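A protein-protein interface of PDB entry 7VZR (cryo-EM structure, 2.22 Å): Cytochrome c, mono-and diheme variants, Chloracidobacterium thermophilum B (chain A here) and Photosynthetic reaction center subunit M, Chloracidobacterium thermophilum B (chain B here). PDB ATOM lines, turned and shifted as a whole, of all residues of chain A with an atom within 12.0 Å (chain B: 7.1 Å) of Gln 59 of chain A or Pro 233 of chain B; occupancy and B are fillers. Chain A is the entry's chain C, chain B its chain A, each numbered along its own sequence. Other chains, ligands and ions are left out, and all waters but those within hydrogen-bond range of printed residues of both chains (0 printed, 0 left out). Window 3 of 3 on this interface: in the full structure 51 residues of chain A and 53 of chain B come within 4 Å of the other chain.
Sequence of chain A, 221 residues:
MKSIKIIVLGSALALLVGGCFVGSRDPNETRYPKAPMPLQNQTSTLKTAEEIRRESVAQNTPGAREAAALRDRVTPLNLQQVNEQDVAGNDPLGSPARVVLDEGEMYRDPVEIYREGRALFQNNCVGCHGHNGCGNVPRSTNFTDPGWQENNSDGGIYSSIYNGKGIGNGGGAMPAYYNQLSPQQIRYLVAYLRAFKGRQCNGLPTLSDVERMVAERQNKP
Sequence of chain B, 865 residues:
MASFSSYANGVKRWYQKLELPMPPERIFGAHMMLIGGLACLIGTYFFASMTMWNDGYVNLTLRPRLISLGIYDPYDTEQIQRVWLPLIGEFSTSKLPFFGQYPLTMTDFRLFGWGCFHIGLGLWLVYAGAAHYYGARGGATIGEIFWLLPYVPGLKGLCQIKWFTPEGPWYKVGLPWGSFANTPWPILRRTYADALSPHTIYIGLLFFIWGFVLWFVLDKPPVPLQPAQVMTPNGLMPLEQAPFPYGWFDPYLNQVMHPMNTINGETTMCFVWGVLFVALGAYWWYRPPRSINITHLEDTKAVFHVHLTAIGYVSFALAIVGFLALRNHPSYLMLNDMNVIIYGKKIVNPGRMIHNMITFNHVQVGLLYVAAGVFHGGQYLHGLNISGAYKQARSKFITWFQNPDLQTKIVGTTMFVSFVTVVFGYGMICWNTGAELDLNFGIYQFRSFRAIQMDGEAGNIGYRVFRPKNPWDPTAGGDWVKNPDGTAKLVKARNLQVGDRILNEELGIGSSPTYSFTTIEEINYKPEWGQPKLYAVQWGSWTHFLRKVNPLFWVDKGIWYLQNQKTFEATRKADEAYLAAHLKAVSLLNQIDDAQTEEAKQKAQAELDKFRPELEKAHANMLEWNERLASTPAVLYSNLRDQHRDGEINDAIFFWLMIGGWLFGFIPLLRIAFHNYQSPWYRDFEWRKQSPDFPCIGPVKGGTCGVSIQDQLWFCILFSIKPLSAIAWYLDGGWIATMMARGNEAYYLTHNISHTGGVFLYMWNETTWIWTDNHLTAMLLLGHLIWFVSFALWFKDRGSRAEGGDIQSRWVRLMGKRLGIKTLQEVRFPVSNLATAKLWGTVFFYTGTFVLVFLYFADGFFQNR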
ATOM      1  N   ARG A  31      27.012  26.006 -28.080  1.00  0.00           N
ATOM      2  CA  ARG A  31      27.043  26.420 -26.735  1.00  0.00           C
ATOM      3  C   ARG A  31      25.623  26.666 -26.288  1.00  0.00           C
ATOM      4  O   ARG A  31      25.442  26.961 -25.238  1.00  0.00           O
ATOM      5  CB  ARG A  31      27.898  27.643 -26.578  1.00  0.00           C
ATOM      6  CG  ARG A  31      29.355  27.393 -26.462  1.00  0.00           C
ATOM      7  CD  ARG A  31      30.156  28.626 -26.119  1.00  0.00           C
ATOM      8  NE  ARG A  31      31.601  28.491 -26.266  1.00  0.00           N
ATOM      9  CZ  ARG A  31      32.311  28.845 -27.257  1.00  0.00           C
ATOM     10  NH1 ARG A  31      31.801  29.409 -28.239  1.00  0.00           N
ATOM     11  NH2 ARG A  31      33.545  28.682 -27.202  1.00  0.00           N
ATOM     12  N   TYR A  32      24.616  26.536 -27.110  1.00  0.00           N
ATOM     13  CA  TYR A  32      23.228  26.804 -26.756  1.00  0.00           C
ATOM     14  C   TYR A  32      22.786  25.966 -25.569  1.00  0.00           C
ATOM     15  O   TYR A  32      23.146  24.806 -25.479  1.00  0.00           O
ATOM     16  CB  TYR A  32      22.310  26.567 -27.945  1.00  0.00           C
ATOM     17  CG  TYR A  32      20.942  27.061 -27.722  1.00  0.00           C
ATOM     18  CD1 TYR A  32      20.654  28.342 -27.921  1.00  0.00           C
ATOM     19  CD2 TYR A  32      19.937  26.228 -27.310  1.00  0.00           C
ATOM     20  CE1 TYR A  32      19.452  28.785 -27.771  1.00  0.00           C
ATOM     21  CE2 TYR A  32      18.724  26.679 -27.137  1.00  0.00           C
ATOM     22  CZ  TYR A  32      18.490  27.967 -27.351  1.00  0.00           C
ATOM     23  OH  TYR A  32      17.277  28.483 -27.194  1.00  0.00           O
ATOM     24  N   PRO A  33      22.167  26.557 -24.580  1.00  0.00           N
ATOM     25  CA  PRO A  33      22.217  25.941 -23.252  1.00  0.00           C
ATOM     26  C   PRO A  33      21.203  24.857 -23.016  1.00  0.00           C
ATOM     27  O   PRO A  33      20.070  24.948 -23.439  1.00  0.00           O
ATOM     28  CB  PRO A  33      22.028  27.138 -22.304  1.00  0.00           C
ATOM     29  CG  PRO A  33      21.859  28.262 -23.075  1.00  0.00           C
ATOM     30  CD  PRO A  33      21.960  28.013 -24.482  1.00  0.00           C
ATOM     31  N   LYS A  34      21.606  23.812 -22.322  1.00  0.00           N
ATOM     32  CA  LYS A  34      20.743  22.712 -21.930  1.00  0.00           C
ATOM     33  C   LYS A  34      19.955  23.111 -20.697  1.00  0.00           C
ATOM     34  O   LYS A  34      20.331  24.026 -20.017  1.00  0.00           O
ATOM     35  CB  LYS A  34      21.564  21.443 -21.710  1.00  0.00           C
ATOM     36  CG  LYS A  34      22.562  21.424 -20.614  1.00  0.00           C
ATOM     37  CD  LYS A  34      22.783  20.067 -20.202  1.00  0.00           C
ATOM     38  CE  LYS A  34      23.829  19.916 -19.182  1.00  0.00           C
ATOM     39  NZ  LYS A  34      23.261  19.638 -17.933  1.00  0.00           N
ATOM     40  N   ALA A  35      18.881  22.426 -20.368  1.00  0.00           N
ATOM     41  CA  ALA A  35      18.169  22.687 -19.122  1.00  0.00           C
ATOM     42  C   ALA A  35      19.016  22.299 -17.922  1.00  0.00           C
ATOM     43  O   ALA A  35      19.902  21.456 -17.999  1.00  0.00           O
ATOM     44  CB  ALA A  35      16.852  21.952 -19.088  1.00  0.00           C
ATOM     45  N   PRO A  36      18.838  22.993 -16.814  1.00  0.00           N
ATOM     46  CA  PRO A  36      19.641  22.727 -15.626  1.00  0.00           C
ATOM     47  C   PRO A  36      19.359  21.389 -14.982  1.00  0.00           C
ATOM     48  O   PRO A  36      18.269  20.841 -15.116  1.00  0.00           O
ATOM     49  CB  PRO A  36      19.265  23.872 -14.691  1.00  0.00           C
ATOM     50  CG  PRO A  36      18.128  24.501 -15.261  1.00  0.00           C
ATOM     51  CD  PRO A  36      18.062  24.221 -16.670  1.00  0.00           C
ATOM     52  N   ALA A  58      13.502  24.923 -28.474  1.00  0.00           N
ATOM     53  CA  ALA A  58      13.644  26.402 -28.302  1.00  0.00           C
ATOM     54  C   ALA A  58      12.652  27.198 -29.158  1.00  0.00           C
ATOM     55  O   ALA A  58      12.081  26.605 -30.093  1.00  0.00           O
ATOM     56  CB  ALA A  58      15.037  26.912 -28.490  1.00  0.00           C
ATOM     57  N   GLN A  59      12.618  28.522 -28.936  1.00  0.00           N
ATOM     58  CA  GLN A  59      11.776  29.509 -29.625  1.00  0.00           C
ATOM     59  C   GLN A  59      11.934  29.667 -31.076  1.00  0.00           C
ATOM     60  O   GLN A  59      12.760  29.096 -31.695  1.00  0.00           O
ATOM     61  CB  GLN A  59      12.105  30.930 -29.156  1.00  0.00           C
ATOM     62  CG  GLN A  59      12.155  31.140 -27.692  1.00  0.00           C
ATOM     63  CD  GLN A  59      13.357  30.483 -27.133  1.00  0.00           C
ATOM     64  OE1 GLN A  59      14.506  30.913 -27.394  1.00  0.00           O
ATOM     65  NE2 GLN A  59      13.136  29.440 -26.370  1.00  0.00           N
ATOM     66  N   ASN A  60      11.224  30.634 -31.623  1.00  0.00           N
ATOM     67  CA  ASN A  60      11.357  30.822 -33.090  1.00  0.00           C
ATOM     68  C   ASN A  60      12.441  31.858 -33.410  1.00  0.00           C
ATOM     69  O   ASN A  60      12.746  32.008 -34.609  1.00  0.00           O
ATOM     70  CB  ASN A  60      10.026  31.220 -33.734  1.00  0.00           C
ATOM     71  CG  ASN A  60       9.001  30.111 -33.658  1.00  0.00           C
ATOM     72  OD1 ASN A  60       9.164  29.068 -34.284  1.00  0.00           O
ATOM     73  ND2 ASN A  60       7.947  30.320 -32.879  1.00  0.00           N
ATOM     74  N   THR A  61      13.016  32.514 -32.399  1.00  0.00           N
ATOM     75  CA  THR A  61      14.011  33.602 -32.643  1.00  0.00           C
ATOM     76  C   THR A  61      15.019  33.161 -33.720  1.00  0.00           C
ATOM     77  O   THR A  61      15.496  32.024 -33.607  1.00  0.00           O
ATOM     78  CB  THR A  61      14.624  34.108 -31.337  1.00  0.00           C
ATOM     79  OG1 THR A  61      15.996  34.413 -31.579  1.00  0.00           O
ATOM     80  CG2 THR A  61      14.524  33.105 -30.210  1.00  0.00           C
ATOM     81  N   PRO A  62      15.393  33.985 -34.737  1.00  0.00           N
ATOM     82  CA  PRO A  62      16.219  33.537 -35.868  1.00  0.00           C
ATOM     83  C   PRO A  62      16.906  32.162 -35.859  1.00  0.00           C
ATOM     84  O   PRO A  62      16.475  31.333 -36.634  1.00  0.00           O
ATOM     85  CB  PRO A  62      17.051  34.771 -36.183  1.00  0.00           C
ATOM     86  CG  PRO A  62      16.115  35.925 -35.855  1.00  0.00           C
ATOM     87  CD  PRO A  62      15.057  35.393 -34.900  1.00  0.00           C
ATOM     88  N   GLY A  63      17.931  31.920 -35.032  1.00  0.00           N
ATOM     89  CA  GLY A  63      18.459  30.559 -35.114  1.00  0.00           C
ATOM     90  C   GLY A  63      18.260  29.612 -33.955  1.00  0.00           C
ATOM     91  O   GLY A  63      19.015  28.663 -33.771  1.00  0.00           O
ATOM     92  N   ALA A  64      17.223  29.843 -33.176  1.00  0.00           N
ATOM     93  CA  ALA A  64      17.148  29.211 -31.883  1.00  0.00           C
ATOM     94  C   ALA A  64      16.704  27.764 -31.994  1.00  0.00           C
ATOM     95  O   ALA A  64      16.992  26.948 -31.110  1.00  0.00           O
ATOM     96  CB  ALA A  64      16.217  30.003 -31.004  1.00  0.00           C
ATOM     97  N   ARG A  65      16.059  27.417 -33.110  1.00  0.00           N
ATOM     98  CA  ARG A  65      15.580  26.064 -33.300  1.00  0.00           C
ATOM     99  C   ARG A  65      16.660  25.157 -33.845  1.00  0.00           C
ATOM    100  O   ARG A  65      16.783  24.021 -33.393  1.00  0.00           O
ATOM    101  CB  ARG A  65      14.337  26.077 -34.172  1.00  0.00           C
ATOM    102  CG  ARG A  65      13.215  25.748 -33.303  1.00  0.00           C
ATOM    103  CD  ARG A  65      11.893  26.339 -33.646  1.00  0.00           C
ATOM    104  NE  ARG A  65      10.974  25.272 -33.963  1.00  0.00           N
ATOM    105  CZ  ARG A  65      10.977  24.686 -35.146  1.00  0.00           C
ATOM    106  NH1 ARG A  65      11.817  25.138 -36.076  1.00  0.00           N
ATOM    107  NH2 ARG A  65      10.140  23.694 -35.401  1.00  0.00           N
ATOM    108  N   GLU A  66      17.458  25.629 -34.778  1.00  0.00           N
ATOM    109  CA  GLU A  66      18.661  24.911 -35.156  1.00  0.00           C
ATOM    110  C   GLU A  66      19.598  24.723 -33.989  1.00  0.00           C
ATOM    111  O   GLU A  66      20.218  23.687 -33.880  1.00  0.00           O
ATOM    112  CB  GLU A  66      19.377  25.637 -36.278  1.00  0.00           C
ATOM    113  CG  GLU A  66      18.535  25.771 -37.463  1.00  0.00           C
ATOM    114  CD  GLU A  66      17.846  27.101 -37.535  1.00  0.00           C
ATOM    115  OE1 GLU A  66      17.251  27.533 -36.529  1.00  0.00           O
ATOM    116  OE2 GLU A  66      17.895  27.745 -38.602  1.00  0.00           O
ATOM    117  N   ALA A  67      19.705  25.687 -33.096  1.00  0.00           N
ATOM    118  CA  ALA A  67      20.634  25.505 -32.004  1.00  0.00           C
ATOM    119  C   ALA A  67      20.108  24.512 -30.999  1.00  0.00           C
ATOM    120  O   ALA A  67      20.867  23.703 -30.504  1.00  0.00           O
ATOM    121  CB  ALA A  67      20.982  26.826 -31.345  1.00  0.00           C
ATOM    122  N   ALA A  68      18.814  24.510 -30.725  1.00  0.00           N
ATOM    123  CA  ALA A  68      18.266  23.533 -29.805  1.00  0.00           C
ATOM    124  C   ALA A  68      18.377  22.117 -30.355  1.00  0.00           C
ATOM    125  O   ALA A  68      18.778  21.208 -29.638  1.00  0.00           O
ATOM    126  CB  ALA A  68      16.830  23.901 -29.475  1.00  0.00           C
ATOM    127  N   ALA A  69      18.024  21.921 -31.627  1.00  0.00           N
ATOM    128  CA  ALA A  69      18.186  20.644 -32.297  1.00  0.00           C
ATOM    129  C   ALA A  69      19.618  20.198 -32.323  1.00  0.00           C
ATOM    130  O   ALA A  69      19.895  19.037 -32.114  1.00  0.00           O
ATOM    131  CB  ALA A  69      17.664  20.720 -33.722  1.00  0.00           C
ATOM    132  N   LEU A  70      20.536  21.089 -32.488  1.00  0.00           N
ATOM    133  CA  LEU A  70      21.910  20.752 -32.397  1.00  0.00           C
ATOM    134  C   LEU A  70      22.347  20.465 -30.972  1.00  0.00           C
ATOM    135  O   LEU A  70      23.077  19.621 -30.816  1.00  0.00           O
ATOM    136  CB  LEU A  70      22.719  21.824 -33.028  1.00  0.00           C
ATOM    137  CG  LEU A  70      24.192  21.695 -33.110  1.00  0.00           C
ATOM    138  CD1 LEU A  70      24.620  20.385 -33.727  1.00  0.00           C
ATOM    139  CD2 LEU A  70      24.690  22.850 -33.921  1.00  0.00           C
ATOM    140  N   ARG A  71      21.841  21.133 -29.941  1.00  0.00           N
ATOM    141  CA  ARG A  71      22.207  20.718 -28.614  1.00  0.00           C
ATOM    142  C   ARG A  71      21.731  19.435 -28.151  1.00  0.00           C
ATOM    143  O   ARG A  71      22.402  18.799 -27.494  1.00  0.00           O
ATOM    144  CB  ARG A  71      22.209  21.739 -27.502  1.00  0.00           C
ATOM    145  CG  ARG A  71      20.943  22.273 -27.147  1.00  0.00           C
ATOM    146  CD  ARG A  71      20.698  22.238 -25.695  1.00  0.00           C
ATOM    147  NE  ARG A  71      19.395  21.723 -25.724  1.00  0.00           N
ATOM    148  CZ  ARG A  71      18.247  22.355 -25.656  1.00  0.00           C
ATOM    149  NH1 ARG A  71      18.121  23.565 -25.390  1.00  0.00           N
ATOM    150  NH2 ARG A  71      17.179  21.678 -25.802  1.00  0.00           N
ATOM    151  N   ASP A  72      20.605  19.045 -28.648  1.00  0.00           N
ATOM    152  CA  ASP A  72      19.968  17.754 -28.466  1.00  0.00           C
ATOM    153  C   ASP A  72      20.792  16.589 -28.983  1.00  0.00           C
ATOM    154  O   ASP A  72      20.652  15.627 -28.481  1.00  0.00           O
ATOM    155  CB  ASP A  72      18.489  17.763 -28.900  1.00  0.00           C
ATOM    156  CG  ASP A  72      17.654  18.618 -28.031  1.00  0.00           C
ATOM    157  OD1 ASP A  72      18.118  19.058 -26.963  1.00  0.00           O
ATOM    158  OD2 ASP A  72      16.494  18.880 -28.357  1.00  0.00           O
ATOM    159  N   ASP B  73      25.435  36.870 -23.419  1.00  0.00           N
ATOM    160  CA  ASP B  73      24.086  36.347 -23.413  1.00  0.00           C
ATOM    161  C   ASP B  73      24.044  34.912 -23.929  1.00  0.00           C
ATOM    162  O   ASP B  73      24.264  34.685 -25.108  1.00  0.00           O
ATOM    163  CB  ASP B  73      23.198  37.256 -24.234  1.00  0.00           C
ATOM    164  CG  ASP B  73      21.761  36.892 -24.200  1.00  0.00           C
ATOM    165  OD1 ASP B  73      21.349  35.861 -23.704  1.00  0.00           O
ATOM    166  OD2 ASP B  73      20.981  37.701 -24.695  1.00  0.00           O
ATOM    167  N   TYR B  75      21.707  32.705 -24.595  1.00  0.00           N
ATOM    168  CA  TYR B  75      20.593  32.366 -25.452  1.00  0.00           C
ATOM    169  C   TYR B  75      20.536  33.188 -26.710  1.00  0.00           C
ATOM    170  O   TYR B  75      19.493  33.284 -27.310  1.00  0.00           O
ATOM    171  CB  TYR B  75      19.284  32.575 -24.701  1.00  0.00           C
ATOM    172  CG  TYR B  75      19.063  31.597 -23.647  1.00  0.00           C
ATOM    173  CD1 TYR B  75      18.564  30.372 -23.942  1.00  0.00           C
ATOM    174  CD2 TYR B  75      19.389  31.868 -22.356  1.00  0.00           C
ATOM    175  CE1 TYR B  75      18.398  29.485 -23.020  1.00  0.00           C
ATOM    176  CE2 TYR B  75      19.217  30.963 -21.420  1.00  0.00           C
ATOM    177  CZ  TYR B  75      18.703  29.771 -21.766  1.00  0.00           C
ATOM    178  OH  TYR B  75      18.494  28.806 -20.862  1.00  0.00           O
ATOM    179  N   ASP B  76      21.625  33.778 -27.101  1.00  0.00           N
ATOM    180  CA  ASP B  76      21.727  34.661 -28.235  1.00  0.00           C
ATOM    181  C   ASP B  76      22.208  33.885 -29.448  1.00  0.00           C
ATOM    182  O   ASP B  76      23.335  33.380 -29.457  1.00  0.00           O
ATOM    183  CB  ASP B  76      22.685  35.764 -27.847  1.00  0.00           C
ATOM    184  CG  ASP B  76      22.694  36.872 -28.780  1.00  0.00           C
ATOM    185  OD1 ASP B  76      22.103  36.790 -29.849  1.00  0.00           O
ATOM    186  OD2 ASP B  76      23.280  37.882 -28.430  1.00  0.00           O
ATOM    187  N   THR B  77      21.364  33.793 -30.457  1.00  0.00           N
ATOM    188  CA  THR B  77      21.593  32.973 -31.620  1.00  0.00           C
ATOM    189  C   THR B  77      21.607  33.720 -32.922  1.00  0.00           C
ATOM    190  O   THR B  77      22.201  33.232 -33.862  1.00  0.00           O
ATOM    191  CB  THR B  77      20.526  31.868 -31.728  1.00  0.00           C
ATOM    192  OG1 THR B  77      19.285  32.346 -31.235  1.00  0.00           O
ATOM    193  CG2 THR B  77      20.891  30.698 -30.931  1.00  0.00           C
ATOM    194  N   MET B 231      12.787  41.734 -20.118  1.00  0.00           N
ATOM    195  CA  MET B 231      12.829  40.935 -21.315  1.00  0.00           C
ATOM    196  C   MET B 231      13.629  39.662 -21.239  1.00  0.00           C
ATOM    197  O   MET B 231      14.691  39.686 -20.877  1.00  0.00           O
ATOM    198  CB  MET B 231      13.418  41.776 -22.390  1.00  0.00           C
ATOM    199  CG  MET B 231      13.395  41.193 -23.771  1.00  0.00           C
ATOM    200  SD  MET B 231      11.702  41.288 -24.325  1.00  0.00           S
ATOM    201  CE  MET B 231      11.411  39.607 -24.572  1.00  0.00           C
ATOM    202  N   THR B 232      13.094  38.521 -21.578  1.00  0.00           N
ATOM    203  CA  THR B 232      13.842  37.259 -21.554  1.00  0.00           C
ATOM    204  C   THR B 232      13.834  36.614 -22.926  1.00  0.00           C
ATOM    205  O   THR B 232      13.203  37.076 -23.772  1.00  0.00           O
ATOM    206  CB  THR B 232      13.320  36.279 -20.459  1.00  0.00           C
ATOM    207  OG1 THR B 232      12.200  35.590 -20.922  1.00  0.00           O
ATOM    208  CG2 THR B 232      12.847  36.985 -19.303  1.00  0.00           C
ATOM    209  N   PRO B 233      14.546  35.519 -23.185  1.00  0.00           N
ATOM    210  CA  PRO B 233      14.420  34.855 -24.495  1.00  0.00           C
ATOM    211  C   PRO B 233      13.022  34.252 -24.774  1.00  0.00           C
ATOM    212  O   PRO B 233      12.751  33.979 -25.837  1.00  0.00           O
ATOM    213  CB  PRO B 233      15.412  33.715 -24.407  1.00  0.00           C
ATOM    214  CG  PRO B 233      16.109  33.893 -23.184  1.00  0.00           C
ATOM    215  CD  PRO B 233      15.319  34.710 -22.270  1.00  0.00           C
ATOM    216  N   ASN B 234      12.197  33.992 -23.794  1.00  0.00           N
ATOM    217  CA  ASN B 234      10.877  33.487 -23.895  1.00  0.00           C
ATOM    218  C   ASN B 234       9.877  34.555 -23.708  1.00  0.00           C
ATOM    219  O   ASN B 234       8.815  34.286 -23.273  1.00  0.00           O
ATOM    220  CB  ASN B 234      10.677  32.479 -22.786  1.00  0.00           C
ATOM    221  CG  ASN B 234      11.069  31.083 -23.204  1.00  0.00           C
ATOM    222  OD1 ASN B 234      10.297  30.418 -23.832  1.00  0.00           O
ATOM    223  ND2 ASN B 234      12.276  30.636 -22.851  1.00  0.00           N
ATOM    224  N   GLY B 235      10.174  35.770 -24.033  1.00  0.00           N
ATOM    225  CA  GLY B 235       9.221  36.828 -23.838  1.00  0.00           C
ATOM    226  C   GLY B 235       9.433  37.707 -22.642  1.00  0.00           C
ATOM    227  O   GLY B 235      10.453  37.671 -22.053  1.00  0.00           O
ATOM    228  N   LEU B 236       8.514  38.597 -22.359  1.00  0.00           N
ATOM    229  CA  LEU B 236       8.631  39.541 -21.293  1.00  0.00           C
ATOM    230  C   LEU B 236       8.018  38.932 -20.073  1.00  0.00           C
ATOM    231  O   LEU B 236       6.877  38.586 -20.063  1.00  0.00           O
ATOM    232  CB  LEU B 236       7.886  40.792 -21.683  1.00  0.00           C
ATOM    233  CG  LEU B 236       8.297  42.173 -21.309  1.00  0.00           C
ATOM    234  CD1 LEU B 236       9.514  42.671 -21.985  1.00  0.00           C
ATOM    235  CD2 LEU B 236       7.187  43.163 -21.510  1.00  0.00           C
ATOM    236  N   MET B 237       8.754  38.860 -19.009  1.00  0.00           N
ATOM    237  CA  MET B 237       8.275  38.266 -17.840  1.00  0.00           C
ATOM    238  C   MET B 237       8.337  39.155 -16.635  1.00  0.00           C
ATOM    239  O   MET B 237       8.809  40.233 -16.727  1.00  0.00           O
ATOM    240  CB  MET B 237       9.163  37.100 -17.629  1.00  0.00           C
ATOM    241  CG  MET B 237       8.775  35.922 -18.418  1.00  0.00           C
ATOM    242  SD  MET B 237       9.826  34.553 -18.065  1.00  0.00           S
ATOM    243  CE  MET B 237       8.778  33.708 -16.934  1.00  0.00           C
ATOM    244  N   PRO B 243      14.178  33.858 -15.038  1.00  0.00           N
ATOM    245  CA  PRO B 243      15.433  33.206 -14.707  1.00  0.00           C
ATOM    246  C   PRO B 243      16.713  34.092 -14.798  1.00  0.00           C
ATOM    247  O   PRO B 243      16.731  34.946 -15.555  1.00  0.00           O
ATOM    248  CB  PRO B 243      15.488  32.037 -15.588  1.00  0.00           C
ATOM    249  CG  PRO B 243      14.585  32.370 -16.643  1.00  0.00           C
ATOM    250  CD  PRO B 243      13.530  33.225 -16.133  1.00  0.00           C
ATOM    251  N   TYR B 246      18.284  37.151 -16.747  1.00  0.00           N
ATOM    252  CA  TYR B 246      17.334  38.155 -16.980  1.00  0.00           C
ATOM    253  C   TYR B 246      16.705  38.690 -15.793  1.00  0.00           C
ATOM    254  O   TYR B 246      16.587  39.801 -15.749  1.00  0.00           O
ATOM    255  CB  TYR B 246      16.327  37.687 -18.052  1.00  0.00           C
ATOM    256  CG  TYR B 246      17.069  36.999 -19.081  1.00  0.00           C
ATOM    257  CD1 TYR B 246      17.762  37.677 -20.022  1.00  0.00           C
ATOM    258  CD2 TYR B 246      17.215  35.660 -19.049  1.00  0.00           C
ATOM    259  CE1 TYR B 246      18.507  37.040 -20.936  1.00  0.00           C
ATOM    260  CE2 TYR B 246      17.968  35.018 -19.947  1.00  0.00           C
ATOM    261  CZ  TYR B 246      18.612  35.749 -20.865  1.00  0.00           C
ATOM    262  OH  TYR B 246      19.350  35.120 -21.687  1.00  0.00           O
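The side-chain carboxylate (OD1) of Asp 73 of chain B lies close to the backbone NH (N) of Tyr 75 of chain B. The backbone NH of Asn 234 of chain B sits close to the side-chain hydroxyl of Thr 232 of chain B (3.3 Å). The backbone carbonyl oxygen (O) of Pro 33 of chain A lies within hydrogen-bond range of the guanidinium group (NH1) of Arg 71 of chain A (3.1 Å).
Among the printed residues, pairs that only touch across the chains: Tyr 32 of chain A with Tyr 75 of chain B, Tyr 32 of chain A with Thr 77 of chain B, Pro 33 of chain A with Tyr 75 of chain B, Gln 59 of chain A with Pro 233 of chain B, Gln 59 of chain A with Asn 234 of chain B, Thr 61 of chain A with Thr 77 of chain B, Gly 63 of chain A with Thr 77 of chain B, Ala 64 of chain A with Thr 77 of chain B and Ala 67 of chain A with Thr 77 of chain B.
Of the printed residues of chain B, Tyr 32 of chain A touches Tyr 75 and Thr 77. Of the printed residues of chain B, Pro 33 of chain A touches Tyr 75 (3.7 Å). Lys 34 of chain A touches none of the printed residues of chain B. Gln 59 of chain A touches just these residues of chain B: Pro 233 and Asn 234. Printed residues of chain B within 4 Å of Ala 64 of chain A: Thr 77 (3.8 Å). Of the printed residues of chain B, Ala 67 of chain A touches Thr 77. Tyr 75 of chain B touches two residues of chain A. No residue of chain A comes within 4 Å of Met 231 of chain B. Of chain A, only Gln 59 comes within 4 Å of Pro 233 of chain B. No residue of chain A comes within 4 Å of Gly 235 of chain B. No residue of chain A comes within 4 Å of Pro 243 of chain B. The nearest residue of chain B that does not touch Gln 59 of chain A is Tyr 75 of chain B (5.4 Å). The nearest residue of chain A that does not touch Pro 233 of chain B is Thr 61 of chain A (4.8 Å).
Of the 13 printed residues of chain B, 4 touch a printed residue of chain A. Hydrophobic or aromatic side chains of chain B that line the printed part of chain A: Tyr 75. Among the printed residues, no Asp or Glu carboxylate lies within 4 Å of a Lys or Arg side-chain nitrogen of the other chain.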
